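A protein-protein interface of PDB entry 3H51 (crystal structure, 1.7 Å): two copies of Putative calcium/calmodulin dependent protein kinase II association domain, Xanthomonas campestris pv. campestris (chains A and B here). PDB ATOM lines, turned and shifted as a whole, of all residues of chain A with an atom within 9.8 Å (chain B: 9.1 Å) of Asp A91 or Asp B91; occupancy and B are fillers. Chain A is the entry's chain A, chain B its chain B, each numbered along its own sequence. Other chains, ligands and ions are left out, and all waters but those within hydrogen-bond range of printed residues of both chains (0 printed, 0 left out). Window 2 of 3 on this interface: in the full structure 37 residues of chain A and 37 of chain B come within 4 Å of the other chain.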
ATOM      1  N   GLU A  18      32.665  26.928  -3.399  1.00  0.00           N
ATOM      2  CA  GLU A  18      31.649  25.882  -3.265  1.00  0.00           C
ATOM      3  C   GLU A  18      31.211  25.707  -1.810  1.00  0.00           C
ATOM      4  O   GLU A  18      30.009  25.634  -1.521  1.00  0.00           O
ATOM      5  CB  GLU A  18      32.155  24.549  -3.846  1.00  0.00           C
ATOM      6  CG  GLU A  18      31.424  24.073  -5.122  1.00  0.00           C
ATOM      7  CD  GLU A  18      30.085  23.345  -4.815  1.00  0.00           C
ATOM      8  OE1 GLU A  18      29.098  24.008  -4.413  1.00  0.00           O
ATOM      9  OE2 GLU A  18      30.019  22.103  -4.983  1.00  0.00           O
ATOM     10  N   VAL A  22      27.373  25.962  -0.347  1.00  0.00           N
ATOM     11  CA  VAL A  22      26.774  24.882   0.461  1.00  0.00           C
ATOM     12  C   VAL A  22      26.352  25.405   1.836  1.00  0.00           C
ATOM     13  O   VAL A  22      25.189  25.175   2.229  1.00  0.00           O
ATOM     14  CB  VAL A  22      27.692  23.637   0.498  1.00  0.00           C
ATOM     15  CG1 VAL A  22      27.227  22.597   1.511  1.00  0.00           C
ATOM     16  CG2 VAL A  22      27.795  23.020  -0.955  1.00  0.00           C
ATOM     17  N   ARG A  88      31.996  19.127   3.295  1.00  0.00           N
ATOM     18  CA  ARG A  88      32.724  18.151   2.499  1.00  0.00           C
ATOM     19  C   ARG A  88      32.038  18.031   1.148  1.00  0.00           C
ATOM     20  O   ARG A  88      30.822  17.830   1.099  1.00  0.00           O
ATOM     21  CB  ARG A  88      32.742  16.812   3.220  1.00  0.00           C
ATOM     22  CG  ARG A  88      33.365  16.873   4.582  1.00  0.00           C
ATOM     23  CD  ARG A  88      34.887  17.124   4.501  1.00  0.00           C
ATOM     24  NE  ARG A  88      35.454  17.216   5.836  1.00  0.00           N
ATOM     25  CZ  ARG A  88      35.698  18.359   6.490  1.00  0.00           C
ATOM     26  NH1 ARG A  88      35.446  19.552   5.935  1.00  0.00           N
ATOM     27  NH2 ARG A  88      36.214  18.318   7.697  1.00  0.00           N
ATOM     28  N   LEU A  89      32.813  18.154   0.089  1.00  0.00           N
ATOM     29  CA  LEU A  89      32.274  18.194  -1.288  1.00  0.00           C
ATOM     30  C   LEU A  89      32.501  16.813  -1.881  1.00  0.00           C
ATOM     31  O   LEU A  89      33.626  16.297  -1.844  1.00  0.00           O
ATOM     32  CB  LEU A  89      32.991  19.300  -2.083  1.00  0.00           C
ATOM     33  CG  LEU A  89      32.887  20.709  -1.444  1.00  0.00           C
ATOM     34  CD1 LEU A  89      33.774  21.732  -2.186  1.00  0.00           C
ATOM     35  CD2 LEU A  89      31.455  21.206  -1.340  1.00  0.00           C
ATOM     36  N   LEU A  90      31.443  16.193  -2.380  1.00  0.00           N
ATOM     37  CA  LEU A  90      31.554  14.858  -2.953  1.00  0.00           C
ATOM     38  C   LEU A  90      31.695  14.974  -4.473  1.00  0.00           C
ATOM     39  O   LEU A  90      32.814  14.956  -4.992  1.00  0.00           O
ATOM     40  CB  LEU A  90      30.353  14.011  -2.555  1.00  0.00           C
ATOM     41  CG  LEU A  90      30.147  13.644  -1.074  1.00  0.00           C
ATOM     42  CD1 LEU A  90      28.685  13.607  -0.723  1.00  0.00           C
ATOM     43  CD2 LEU A  90      30.815  12.304  -0.797  1.00  0.00           C
ATOM     44  N   ASP A  91      30.578  15.143  -5.180  1.00  0.00           N
ATOM     45  CA  ASP A  91      30.589  15.281  -6.645  1.00  0.00           C
ATOM     46  C   ASP A  91      31.005  16.723  -6.981  1.00  0.00           C
ATOM     47  O   ASP A  91      31.772  17.353  -6.229  1.00  0.00           O
ATOM     48  CB  ASP A  91      29.185  14.968  -7.225  1.00  0.00           C
ATOM     49  N   ASP A  92      30.512  17.224  -8.116  1.00  0.00           N
ATOM     50  CA  ASP A  92      30.253  18.657  -8.307  1.00  0.00           C
ATOM     51  C   ASP A  92      28.790  18.922  -7.874  1.00  0.00           C
ATOM     52  O   ASP A  92      28.350  20.081  -7.723  1.00  0.00           O
ATOM     53  CB  ASP A  92      30.467  19.067  -9.784  1.00  0.00           C
ATOM     54  N   ASP A  93      28.046  17.832  -7.677  1.00  0.00           N
ATOM     55  CA  ASP A  93      26.624  17.910  -7.426  1.00  0.00           C
ATOM     56  C   ASP A  93      26.187  17.198  -6.131  1.00  0.00           C
ATOM     57  O   ASP A  93      25.015  16.891  -5.975  1.00  0.00           O
ATOM     58  CB  ASP A  93      25.887  17.310  -8.618  1.00  0.00           C
ATOM     59  CG  ASP A  93      25.895  18.226  -9.844  1.00  0.00           C
ATOM     60  OD1 ASP A  93      26.794  19.086 -10.003  1.00  0.00           O
ATOM     61  OD2 ASP A  93      24.982  18.068 -10.658  1.00  0.00           O
ATOM     62  N   SER A  94      27.114  16.912  -5.207  1.00  0.00           N
ATOM     63  CA  SER A  94      26.689  16.535  -3.867  1.00  0.00           C
ATOM     64  C   SER A  94      27.648  17.010  -2.783  1.00  0.00           C
ATOM     65  O   SER A  94      28.831  17.125  -2.998  1.00  0.00           O
ATOM     66  CB  SER A  94      26.366  15.033  -3.751  1.00  0.00           C
ATOM     67  OG  SER A  94      27.530  14.239  -3.694  1.00  0.00           O
ATOM     68  N   ALA A  95      27.091  17.319  -1.621  1.00  0.00           N
ATOM     69  CA  ALA A  95      27.849  17.892  -0.492  1.00  0.00           C
ATOM     70  C   ALA A  95      27.262  17.551   0.851  1.00  0.00           C
ATOM     71  O   ALA A  95      26.062  17.300   0.968  1.00  0.00           O
ATOM     72  CB  ALA A  95      27.919  19.389  -0.631  1.00  0.00           C
ATOM     73  N   VAL A  96      28.106  17.573   1.890  1.00  0.00           N
ATOM     74  CA  VAL A  96      27.668  17.375   3.259  1.00  0.00           C
ATOM     75  C   VAL A  96      28.087  18.549   4.134  1.00  0.00           C
ATOM     76  O   VAL A  96      29.280  18.899   4.189  1.00  0.00           O
ATOM     77  CB  VAL A  96      28.251  16.090   3.882  1.00  0.00           C
ATOM     78  CG1 VAL A  96      27.684  15.847   5.294  1.00  0.00           C
ATOM     79  CG2 VAL A  96      28.005  14.895   2.949  1.00  0.00           C
ATOM     80  N   VAL A 122      22.858  16.367   3.927  1.00  0.00           N
ATOM     81  CA  VAL A 122      23.453  15.850   2.701  1.00  0.00           C
ATOM     82  C   VAL A 122      22.576  16.426   1.589  1.00  0.00           C
ATOM     83  O   VAL A 122      21.313  16.227   1.573  1.00  0.00           O
ATOM     84  CB  VAL A 122      23.466  14.322   2.584  1.00  0.00           C
ATOM     85  CG1 VAL A 122      24.212  13.873   1.311  1.00  0.00           C
ATOM     86  CG2 VAL A 122      24.133  13.664   3.827  1.00  0.00           C
ATOM     87  N   TYR A 123      23.257  17.213   0.754  1.00  0.00           N
ATOM     88  CA  TYR A 123      22.629  17.836  -0.398  1.00  0.00           C
ATOM     89  C   TYR A 123      23.026  17.157  -1.740  1.00  0.00           C
ATOM     90  O   TYR A 123      24.178  16.722  -1.972  1.00  0.00           O
ATOM     91  CB  TYR A 123      22.988  19.293  -0.494  1.00  0.00           C
ATOM     92  CG  TYR A 123      22.782  20.110   0.739  1.00  0.00           C
ATOM     93  CD1 TYR A 123      21.525  20.594   1.071  1.00  0.00           C
ATOM     94  CD2 TYR A 123      23.841  20.464   1.531  1.00  0.00           C
ATOM     95  CE1 TYR A 123      21.342  21.413   2.172  1.00  0.00           C
ATOM     96  CE2 TYR A 123      23.658  21.232   2.695  1.00  0.00           C
ATOM     97  CZ  TYR A 123      22.385  21.717   2.993  1.00  0.00           C
ATOM     98  OH  TYR A 123      22.185  22.497   4.127  1.00  0.00           O
ATOM     99  N   GLU A 124      22.073  17.146  -2.672  1.00  0.00           N
ATOM    100  CA  GLU A 124      22.337  16.630  -3.996  1.00  0.00           C
ATOM    101  C   GLU A 124      21.799  17.688  -4.951  1.00  0.00           C
ATOM    102  O   GLU A 124      20.703  18.140  -4.747  1.00  0.00           O
ATOM    103  CB  GLU A 124      21.609  15.307  -4.191  1.00  0.00           C
ATOM    104  CG  GLU A 124      21.740  14.732  -5.605  1.00  0.00           C
ATOM    105  CD  GLU A 124      21.132  13.357  -5.702  1.00  0.00           C
ATOM    106  OE1 GLU A 124      20.051  13.140  -5.112  1.00  0.00           O
ATOM    107  OE2 GLU A 124      21.769  12.485  -6.330  1.00  0.00           O
ATOM    108  N   LYS A 125      22.580  18.087  -5.955  1.00  0.00           N
ATOM    109  CA  LYS A 125      22.105  19.074  -6.939  1.00  0.00           C
ATOM    110  C   LYS A 125      21.478  18.352  -8.133  1.00  0.00           C
ATOM    111  O   LYS A 125      22.154  17.567  -8.802  1.00  0.00           O
ATOM    112  CB  LYS A 125      23.247  20.009  -7.388  1.00  0.00           C
ATOM    113  CG  LYS A 125      22.771  21.172  -8.241  1.00  0.00           C
ATOM    114  CD  LYS A 125      23.599  22.433  -8.053  1.00  0.00           C
ATOM    115  CE  LYS A 125      24.930  22.338  -8.734  1.00  0.00           C
ATOM    116  NZ  LYS A 125      25.703  23.588  -8.508  1.00  0.00           N
ATOM    117  N   ARG A 126      20.194  18.592  -8.362  1.00  0.00           N
ATOM    118  CA  ARG A 126      19.473  18.015  -9.513  1.00  0.00           C
ATOM    119  C   ARG A 126      18.814  19.124 -10.301  1.00  0.00           C
ATOM    120  O   ARG A 126      18.145  19.980  -9.720  1.00  0.00           O
ATOM    121  CB  ARG A 126      18.358  17.082  -9.066  1.00  0.00           C
ATOM    122  CG  ARG A 126      18.719  16.151  -7.975  1.00  0.00           C
ATOM    123  CD  ARG A 126      17.480  15.635  -7.298  1.00  0.00           C
ATOM    124  NE  ARG A 126      17.776  14.452  -6.489  1.00  0.00           N
ATOM    125  CZ  ARG A 126      16.853  13.632  -5.988  1.00  0.00           C
ATOM    126  NH1 ARG A 126      15.545  13.854  -6.198  1.00  0.00           N
ATOM    127  NH2 ARG A 126      17.253  12.580  -5.276  1.00  0.00           N
ATOM    128  N   TRP A 130      19.964  22.555  -5.614  1.00  0.00           N
ATOM    129  CA  TRP A 130      20.278  21.747  -4.442  1.00  0.00           C
ATOM    130  C   TRP A 130      19.026  21.351  -3.664  1.00  0.00           C
ATOM    131  O   TRP A 130      18.169  22.190  -3.382  1.00  0.00           O
ATOM    132  CB  TRP A 130      21.171  22.526  -3.511  1.00  0.00           C
ATOM    133  CG  TRP A 130      22.543  22.824  -3.996  1.00  0.00           C
ATOM    134  CD1 TRP A 130      23.022  24.041  -4.435  1.00  0.00           C
ATOM    135  CD2 TRP A 130      23.658  21.921  -4.033  1.00  0.00           C
ATOM    136  NE1 TRP A 130      24.360  23.934  -4.736  1.00  0.00           N
ATOM    137  CE2 TRP A 130      24.778  22.652  -4.481  1.00  0.00           C
ATOM    138  CE3 TRP A 130      23.819  20.562  -3.726  1.00  0.00           C
ATOM    139  CZ2 TRP A 130      26.026  22.066  -4.645  1.00  0.00           C
ATOM    140  CZ3 TRP A 130      25.060  20.000  -3.851  1.00  0.00           C
ATOM    141  CH2 TRP A 130      26.144  20.735  -4.317  1.00  0.00           C
ATOM    142  N   ILE A 133      18.906  15.417   0.611  1.00  0.00           N
ATOM    143  CA  ILE A 133      18.675  13.976   0.562  1.00  0.00           C
ATOM    144  C   ILE A 133      18.712  13.272   1.921  1.00  0.00           C
ATOM    145  O   ILE A 133      18.086  12.243   2.111  1.00  0.00           O
ATOM    146  CB  ILE A 133      19.652  13.294  -0.454  1.00  0.00           C
ATOM    147  CG1 ILE A 133      19.103  11.922  -0.902  1.00  0.00           C
ATOM    148  CG2 ILE A 133      21.081  13.293   0.066  1.00  0.00           C
ATOM    149  CD1 ILE A 133      17.955  11.996  -1.915  1.00  0.00           C
ATOM    150  N   GLU B  18      23.370  -2.931  -6.427  1.00  0.00           N
ATOM    151  CA  GLU B  18      24.387  -1.958  -5.955  1.00  0.00           C
ATOM    152  C   GLU B  18      24.005  -1.174  -4.673  1.00  0.00           C
ATOM    153  O   GLU B  18      24.873  -0.572  -3.965  1.00  0.00           O
ATOM    154  CB  GLU B  18      24.633  -0.934  -7.055  1.00  0.00           C
ATOM    155  N   GLU B  21      25.689  -3.436  -2.293  1.00  0.00           N
ATOM    156  CA  GLU B  21      27.092  -3.050  -2.040  1.00  0.00           C
ATOM    157  C   GLU B  21      27.198  -2.015  -0.909  1.00  0.00           C
ATOM    158  O   GLU B  21      27.953  -2.201   0.055  1.00  0.00           O
ATOM    159  CB  GLU B  21      27.758  -2.480  -3.300  1.00  0.00           C
ATOM    160  CG  GLU B  21      29.273  -2.490  -3.226  1.00  0.00           C
ATOM    161  CD  GLU B  21      29.956  -1.757  -4.373  1.00  0.00           C
ATOM    162  OE1 GLU B  21      29.298  -1.367  -5.367  1.00  0.00           O
ATOM    163  OE2 GLU B  21      31.174  -1.570  -4.262  1.00  0.00           O
ATOM    164  N   VAL B  22      26.425  -0.941  -1.041  1.00  0.00           N
ATOM    165  CA  VAL B  22      26.421   0.130  -0.055  1.00  0.00           C
ATOM    166  C   VAL B  22      25.914  -0.399   1.299  1.00  0.00           C
ATOM    167  O   VAL B  22      26.549  -0.180   2.338  1.00  0.00           O
ATOM    168  CB  VAL B  22      25.573   1.322  -0.512  1.00  0.00           C
ATOM    169  CG1 VAL B  22      25.420   2.363   0.652  1.00  0.00           C
ATOM    170  CG2 VAL B  22      26.238   1.960  -1.717  1.00  0.00           C
ATOM    171  N   ARG B  88      20.279   5.724  -0.560  1.00  0.00           N
ATOM    172  CA  ARG B  88      20.161   6.703  -1.633  1.00  0.00           C
ATOM    173  C   ARG B  88      21.520   6.817  -2.301  1.00  0.00           C
ATOM    174  O   ARG B  88      22.490   7.167  -1.681  1.00  0.00           O
ATOM    175  CB  ARG B  88      19.725   8.055  -1.102  1.00  0.00           C
ATOM    176  CG  ARG B  88      18.383   8.059  -0.345  1.00  0.00           C
ATOM    177  CD  ARG B  88      17.247   7.734  -1.289  1.00  0.00           C
ATOM    178  NE  ARG B  88      15.962   7.717  -0.569  1.00  0.00           N
ATOM    179  CZ  ARG B  88      15.369   6.641  -0.063  1.00  0.00           C
ATOM    180  NH1 ARG B  88      15.887   5.435  -0.238  1.00  0.00           N
ATOM    181  NH2 ARG B  88      14.194   6.777   0.567  1.00  0.00           N
ATOM    182  N   LEU B  89      21.554   6.503  -3.598  1.00  0.00           N
ATOM    183  CA  LEU B  89      22.823   6.573  -4.382  1.00  0.00           C
ATOM    184  C   LEU B  89      22.925   7.975  -4.971  1.00  0.00           C
ATOM    185  O   LEU B  89      22.010   8.408  -5.662  1.00  0.00           O
ATOM    186  CB  LEU B  89      22.787   5.522  -5.480  1.00  0.00           C
ATOM    187  CG  LEU B  89      22.446   4.098  -5.023  1.00  0.00           C
ATOM    188  CD1 LEU B  89      22.505   3.207  -6.248  1.00  0.00           C
ATOM    189  CD2 LEU B  89      23.359   3.568  -3.906  1.00  0.00           C
ATOM    190  N   LEU B  90      24.012   8.686  -4.744  1.00  0.00           N
ATOM    191  CA  LEU B  90      24.122  10.031  -5.305  1.00  0.00           C
ATOM    192  C   LEU B  90      24.738   9.984  -6.709  1.00  0.00           C
ATOM    193  O   LEU B  90      24.124  10.417  -7.685  1.00  0.00           O
ATOM    194  CB  LEU B  90      24.909  10.926  -4.363  1.00  0.00           C
ATOM    195  CG  LEU B  90      24.312  10.903  -2.937  1.00  0.00           C
ATOM    196  CD1 LEU B  90      25.286  11.474  -1.932  1.00  0.00           C
ATOM    197  CD2 LEU B  90      23.003  11.639  -2.922  1.00  0.00           C
ATOM    198  N   ASP B  91      25.939   9.441  -6.809  1.00  0.00           N
ATOM    199  CA  ASP B  91      26.536   9.114  -8.110  1.00  0.00           C
ATOM    200  C   ASP B  91      27.135   7.702  -8.002  1.00  0.00           C
ATOM    201  O   ASP B  91      26.922   6.998  -6.980  1.00  0.00           O
ATOM    202  CB  ASP B  91      27.592  10.181  -8.521  1.00  0.00           C
ATOM    203  CG  ASP B  91      28.580  10.550  -7.377  1.00  0.00           C
ATOM    204  OD1 ASP B  91      28.214  11.404  -6.525  1.00  0.00           O
ATOM    205  OD2 ASP B  91      29.733  10.024  -7.356  1.00  0.00           O
ATOM    206  N   ASP B  92      27.912   7.304  -9.018  1.00  0.00           N
ATOM    207  CA  ASP B  92      28.709   6.076  -8.955  1.00  0.00           C
ATOM    208  C   ASP B  92      29.561   6.009  -7.673  1.00  0.00           C
ATOM    209  O   ASP B  92      29.867   4.914  -7.175  1.00  0.00           O
ATOM    210  CB  ASP B  92      29.626   5.955 -10.189  1.00  0.00           C
ATOM    211  N   ASP B  93      29.956   7.172  -7.166  1.00  0.00           N
ATOM    212  CA  ASP B  93      30.975   7.228  -6.127  1.00  0.00           C
ATOM    213  C   ASP B  93      30.530   7.883  -4.826  1.00  0.00           C
ATOM    214  O   ASP B  93      31.356   8.200  -3.978  1.00  0.00           O
ATOM    215  CB  ASP B  93      32.210   7.957  -6.651  1.00  0.00           C
ATOM    216  CG  ASP B  93      32.879   7.236  -7.819  1.00  0.00           C
ATOM    217  OD1 ASP B  93      32.787   5.980  -7.956  1.00  0.00           O
ATOM    218  OD2 ASP B  93      33.505   7.971  -8.603  1.00  0.00           O
ATOM    219  N   SER B  94      29.234   8.110  -4.656  1.00  0.00           N
ATOM    220  CA  SER B  94      28.774   8.478  -3.350  1.00  0.00           C
ATOM    221  C   SER B  94      27.358   7.949  -3.043  1.00  0.00           C
ATOM    222  O   SER B  94      26.529   7.755  -3.933  1.00  0.00           O
ATOM    223  CB  SER B  94      28.877  10.000  -3.141  1.00  0.00           C
ATOM    224  OG  SER B  94      28.036  10.716  -4.039  1.00  0.00           O
ATOM    225  N   ALA B  95      27.103   7.716  -1.760  1.00  0.00           N
ATOM    226  CA  ALA B  95      25.832   7.108  -1.340  1.00  0.00           C
ATOM    227  C   ALA B  95      25.553   7.439   0.132  1.00  0.00           C
ATOM    228  O   ALA B  95      26.475   7.729   0.905  1.00  0.00           O
ATOM    229  CB  ALA B  95      25.859   5.583  -1.577  1.00  0.00           C
ATOM    230  N   VAL B  96      24.269   7.366   0.495  1.00  0.00           N
ATOM    231  CA  VAL B  96      23.806   7.533   1.865  1.00  0.00           C
ATOM    232  C   VAL B  96      22.967   6.333   2.304  1.00  0.00           C
ATOM    233  O   VAL B  96      21.985   5.959   1.646  1.00  0.00           O
ATOM    234  CB  VAL B  96      22.903   8.729   2.031  1.00  0.00           C
ATOM    235  CG1 VAL B  96      22.682   8.974   3.565  1.00  0.00           C
ATOM    236  CG2 VAL B  96      23.512   9.932   1.373  1.00  0.00           C
ATOM    237  N   VAL B 122      27.319   8.477   5.239  1.00  0.00           N
ATOM    238  CA  VAL B 122      27.537   8.991   3.912  1.00  0.00           C
ATOM    239  C   VAL B 122      28.890   8.434   3.488  1.00  0.00           C
ATOM    240  O   VAL B 122      29.900   8.586   4.193  1.00  0.00           O
ATOM    241  CB  VAL B 122      27.555  10.514   3.860  1.00  0.00           C
ATOM    242  CG1 VAL B 122      27.768  11.014   2.440  1.00  0.00           C
ATOM    243  CG2 VAL B 122      26.268  11.049   4.525  1.00  0.00           C
ATOM    244  N   TYR B 123      28.859   7.749   2.351  1.00  0.00           N
ATOM    245  CA  TYR B 123      30.069   7.144   1.815  1.00  0.00           C
ATOM    246  C   TYR B 123      30.538   7.788   0.514  1.00  0.00           C
ATOM    247  O   TYR B 123      29.734   8.198  -0.342  1.00  0.00           O
ATOM    248  CB  TYR B 123      29.849   5.669   1.487  1.00  0.00           C
ATOM    249  CG  TYR B 123      29.301   4.825   2.591  1.00  0.00           C
ATOM    250  CD1 TYR B 123      30.132   4.348   3.628  1.00  0.00           C
ATOM    251  CD2 TYR B 123      27.948   4.453   2.606  1.00  0.00           C
ATOM    252  CE1 TYR B 123      29.659   3.539   4.625  1.00  0.00           C
ATOM    253  CE2 TYR B 123      27.462   3.617   3.622  1.00  0.00           C
ATOM    254  CZ  TYR B 123      28.318   3.176   4.636  1.00  0.00           C
ATOM    255  OH  TYR B 123      27.888   2.343   5.653  1.00  0.00           O
ATOM    256  N   GLU B 124      31.858   7.770   0.319  1.00  0.00           N
ATOM    257  CA  GLU B 124      32.461   8.209  -0.927  1.00  0.00           C
ATOM    258  C   GLU B 124      33.442   7.149  -1.352  1.00  0.00           C
ATOM    259  O   GLU B 124      34.235   6.699  -0.544  1.00  0.00           O
ATOM    260  CB  GLU B 124      33.192   9.532  -0.741  1.00  0.00           C
ATOM    261  CG  GLU B 124      33.937   9.939  -1.996  1.00  0.00           C
ATOM    262  CD  GLU B 124      34.306  11.410  -2.074  1.00  0.00           C
ATOM    263  OE1 GLU B 124      34.987  11.927  -1.162  1.00  0.00           O
ATOM    264  OE2 GLU B 124      33.926  12.034  -3.102  1.00  0.00           O
ATOM    265  N   LYS B 125      33.386   6.771  -2.624  1.00  0.00           N
ATOM    266  CA  LYS B 125      34.333   5.815  -3.182  1.00  0.00           C
ATOM    267  C   LYS B 125      35.566   6.579  -3.669  1.00  0.00           C
ATOM    268  O   LYS B 125      35.471   7.446  -4.539  1.00  0.00           O
ATOM    269  CB  LYS B 125      33.699   5.013  -4.322  1.00  0.00           C
ATOM    270  CG  LYS B 125      34.642   3.970  -4.872  1.00  0.00           C
ATOM    271  CD  LYS B 125      33.978   2.607  -5.044  1.00  0.00           C
ATOM    272  CE  LYS B 125      32.854   2.632  -6.040  1.00  0.00           C
ATOM    273  NZ  LYS B 125      32.631   1.264  -6.638  1.00  0.00           N
ATOM    274  N   ARG B 126      36.708   6.241  -3.088  1.00  0.00           N
ATOM    275  CA  ARG B 126      37.986   6.823  -3.455  1.00  0.00           C
ATOM    276  C   ARG B 126      38.957   5.728  -3.826  1.00  0.00           C
ATOM    277  O   ARG B 126      39.175   4.805  -3.037  1.00  0.00           O
ATOM    278  CB  ARG B 126      38.574   7.593  -2.284  1.00  0.00           C
ATOM    279  CG  ARG B 126      37.718   8.757  -1.838  1.00  0.00           C
ATOM    280  CD  ARG B 126      38.407   9.524  -0.735  1.00  0.00           C
ATOM    281  NE  ARG B 126      37.571  10.620  -0.252  1.00  0.00           N
ATOM    282  CZ  ARG B 126      37.927  11.450   0.722  1.00  0.00           C
ATOM    283  NH1 ARG B 126      39.087  11.313   1.328  1.00  0.00           N
ATOM    284  NH2 ARG B 126      37.102  12.426   1.072  1.00  0.00           N
ATOM    285  N   TRP B 130      35.313   2.421  -0.680  1.00  0.00           N
ATOM    286  CA  TRP B 130      34.283   3.237  -0.049  1.00  0.00           C
ATOM    287  C   TRP B 130      34.728   3.648   1.377  1.00  0.00           C
ATOM    288  O   TRP B 130      35.074   2.792   2.209  1.00  0.00           O
ATOM    289  CB  TRP B 130      32.999   2.446   0.115  1.00  0.00           C
ATOM    290  CG  TRP B 130      32.182   2.180  -1.117  1.00  0.00           C
ATOM    291  CD1 TRP B 130      32.026   0.976  -1.754  1.00  0.00           C
ATOM    292  CD2 TRP B 130      31.351   3.115  -1.810  1.00  0.00           C
ATOM    293  NE1 TRP B 130      31.127   1.109  -2.790  1.00  0.00           N
ATOM    294  CE2 TRP B 130      30.699   2.407  -2.847  1.00  0.00           C
ATOM    295  CE3 TRP B 130      31.062   4.467  -1.632  1.00  0.00           C
ATOM    296  CZ2 TRP B 130      29.818   3.021  -3.724  1.00  0.00           C
ATOM    297  CZ3 TRP B 130      30.173   5.075  -2.495  1.00  0.00           C
ATOM    298  CH2 TRP B 130      29.579   4.351  -3.548  1.00  0.00           C
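Of chain B, only Asp B91 (3.8 Å) comes within 4 Å of Asp A91. Of chain A, only Asp A91 comes within 4 Å of Asp B91. Of chain B, only Leu B90 (3.97 Å) and Ser B94 (3.6 Å) come within 4 Å of Ser A94. No residue of chain A comes within 4 Å of Asp B92. Of chain A, only Leu A90 and Ser A94 come within 4 Å of Ser B94. Printed residues of chain B within 4 Å of Val A122: Val B122 (3.4 Å). Printed residues of chain A within 4 Å of Arg B88: Ile A133 (3.9 Å). Printed residues of chain B within 4 Å of Leu A90: Ser B94 (3.8 Å) and Glu B124 (3.7 Å). Glu B21 touches none of the printed residues of chain A. Ala A95 touches none of the printed residues of chain B. The nearest residue of chain B that does not touch Asp A91 is Glu B124 (5.0 Å). The nearest residue of chain A that does not touch Asp B91 is Ser A94 (4.1 Å). The nearest printed residue of chain B that does not touch Val A96 is Leu B90 (6.6 Å).
Leu A90 touches Glu B124, and with the chains exchanged Glu A124 touches Leu B90. Ser A94 touches its own counterpart, Ser B94. Val A96 touches Val B122, but with the chains exchanged Val A122 does not touch Val B96 (4.003 Å). Val A122 touches its own counterpart, Val B122. 17 positions are printed for both chains. Of the 10 pairs that touch across the chains among the printed residues, 7 have their exchanged pair printed and touching as well.
Hydrophobic or aromatic side chains of chain A that line the printed part of chain B: Leu A90, Val A96, Val A122 and Ile A133. Hydrophobic or aromatic side chains of chain B that line the printed part of chain A: Leu B90 and Val B122. Among the printed residues, 10 pairs touch across the chains. Among the printed residues, no Asp or Glu carboxylate lies within 4 Å of a Lys or Arg side-chain nitrogen of the other chain.
Among the printed residues, pairs that only touch across the chains: Leu A90 with Ser B94 (3.8 Å), Leu A90 with Glu B124 (3.7 Å), Asp A91 with Asp B91 (3.8 Å), Ser A94 with Leu B90 (3.97 Å), Ser A94 with Ser B94 (3.6 Å), Val A96 with Val B122 (3.9 Å), Val A122 with Val B122 (3.4 Å), Ile A133 with Arg B88 (3.9 Å) and Ile A133 with Leu B90 (3.9 Å).
The side-chain carboxylate (OE2) of Glu A124 lies close to the backbone carbonyl oxygen (O) of Leu B90 (3.4 Å).
O of Arg A88 lies within hydrogen-bond range of N of Val A96 (2.8 Å). O of Val A122 sits at hydrogen-bond distance from N of Ile A133 (2.7 Å). The side-chain carboxylate (OE1) of Glu A124 lies within salt-bridge range of the guanidinium group (NH2) of Arg A126, 2.9 Å away. The backbone carbonyl oxygen (O) of Val B96 sits at hydrogen-bond distance from the backbone NH (N) of Arg B88, 2.8 Å away. The side-chain carboxylate of Asp B91 is in hydrogen-bond range of the backbone NH of Asp B93 (2.9 Å). NE of Arg B126 lies within salt-bridge range of OE1 of Glu B124 (3.0 Å).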
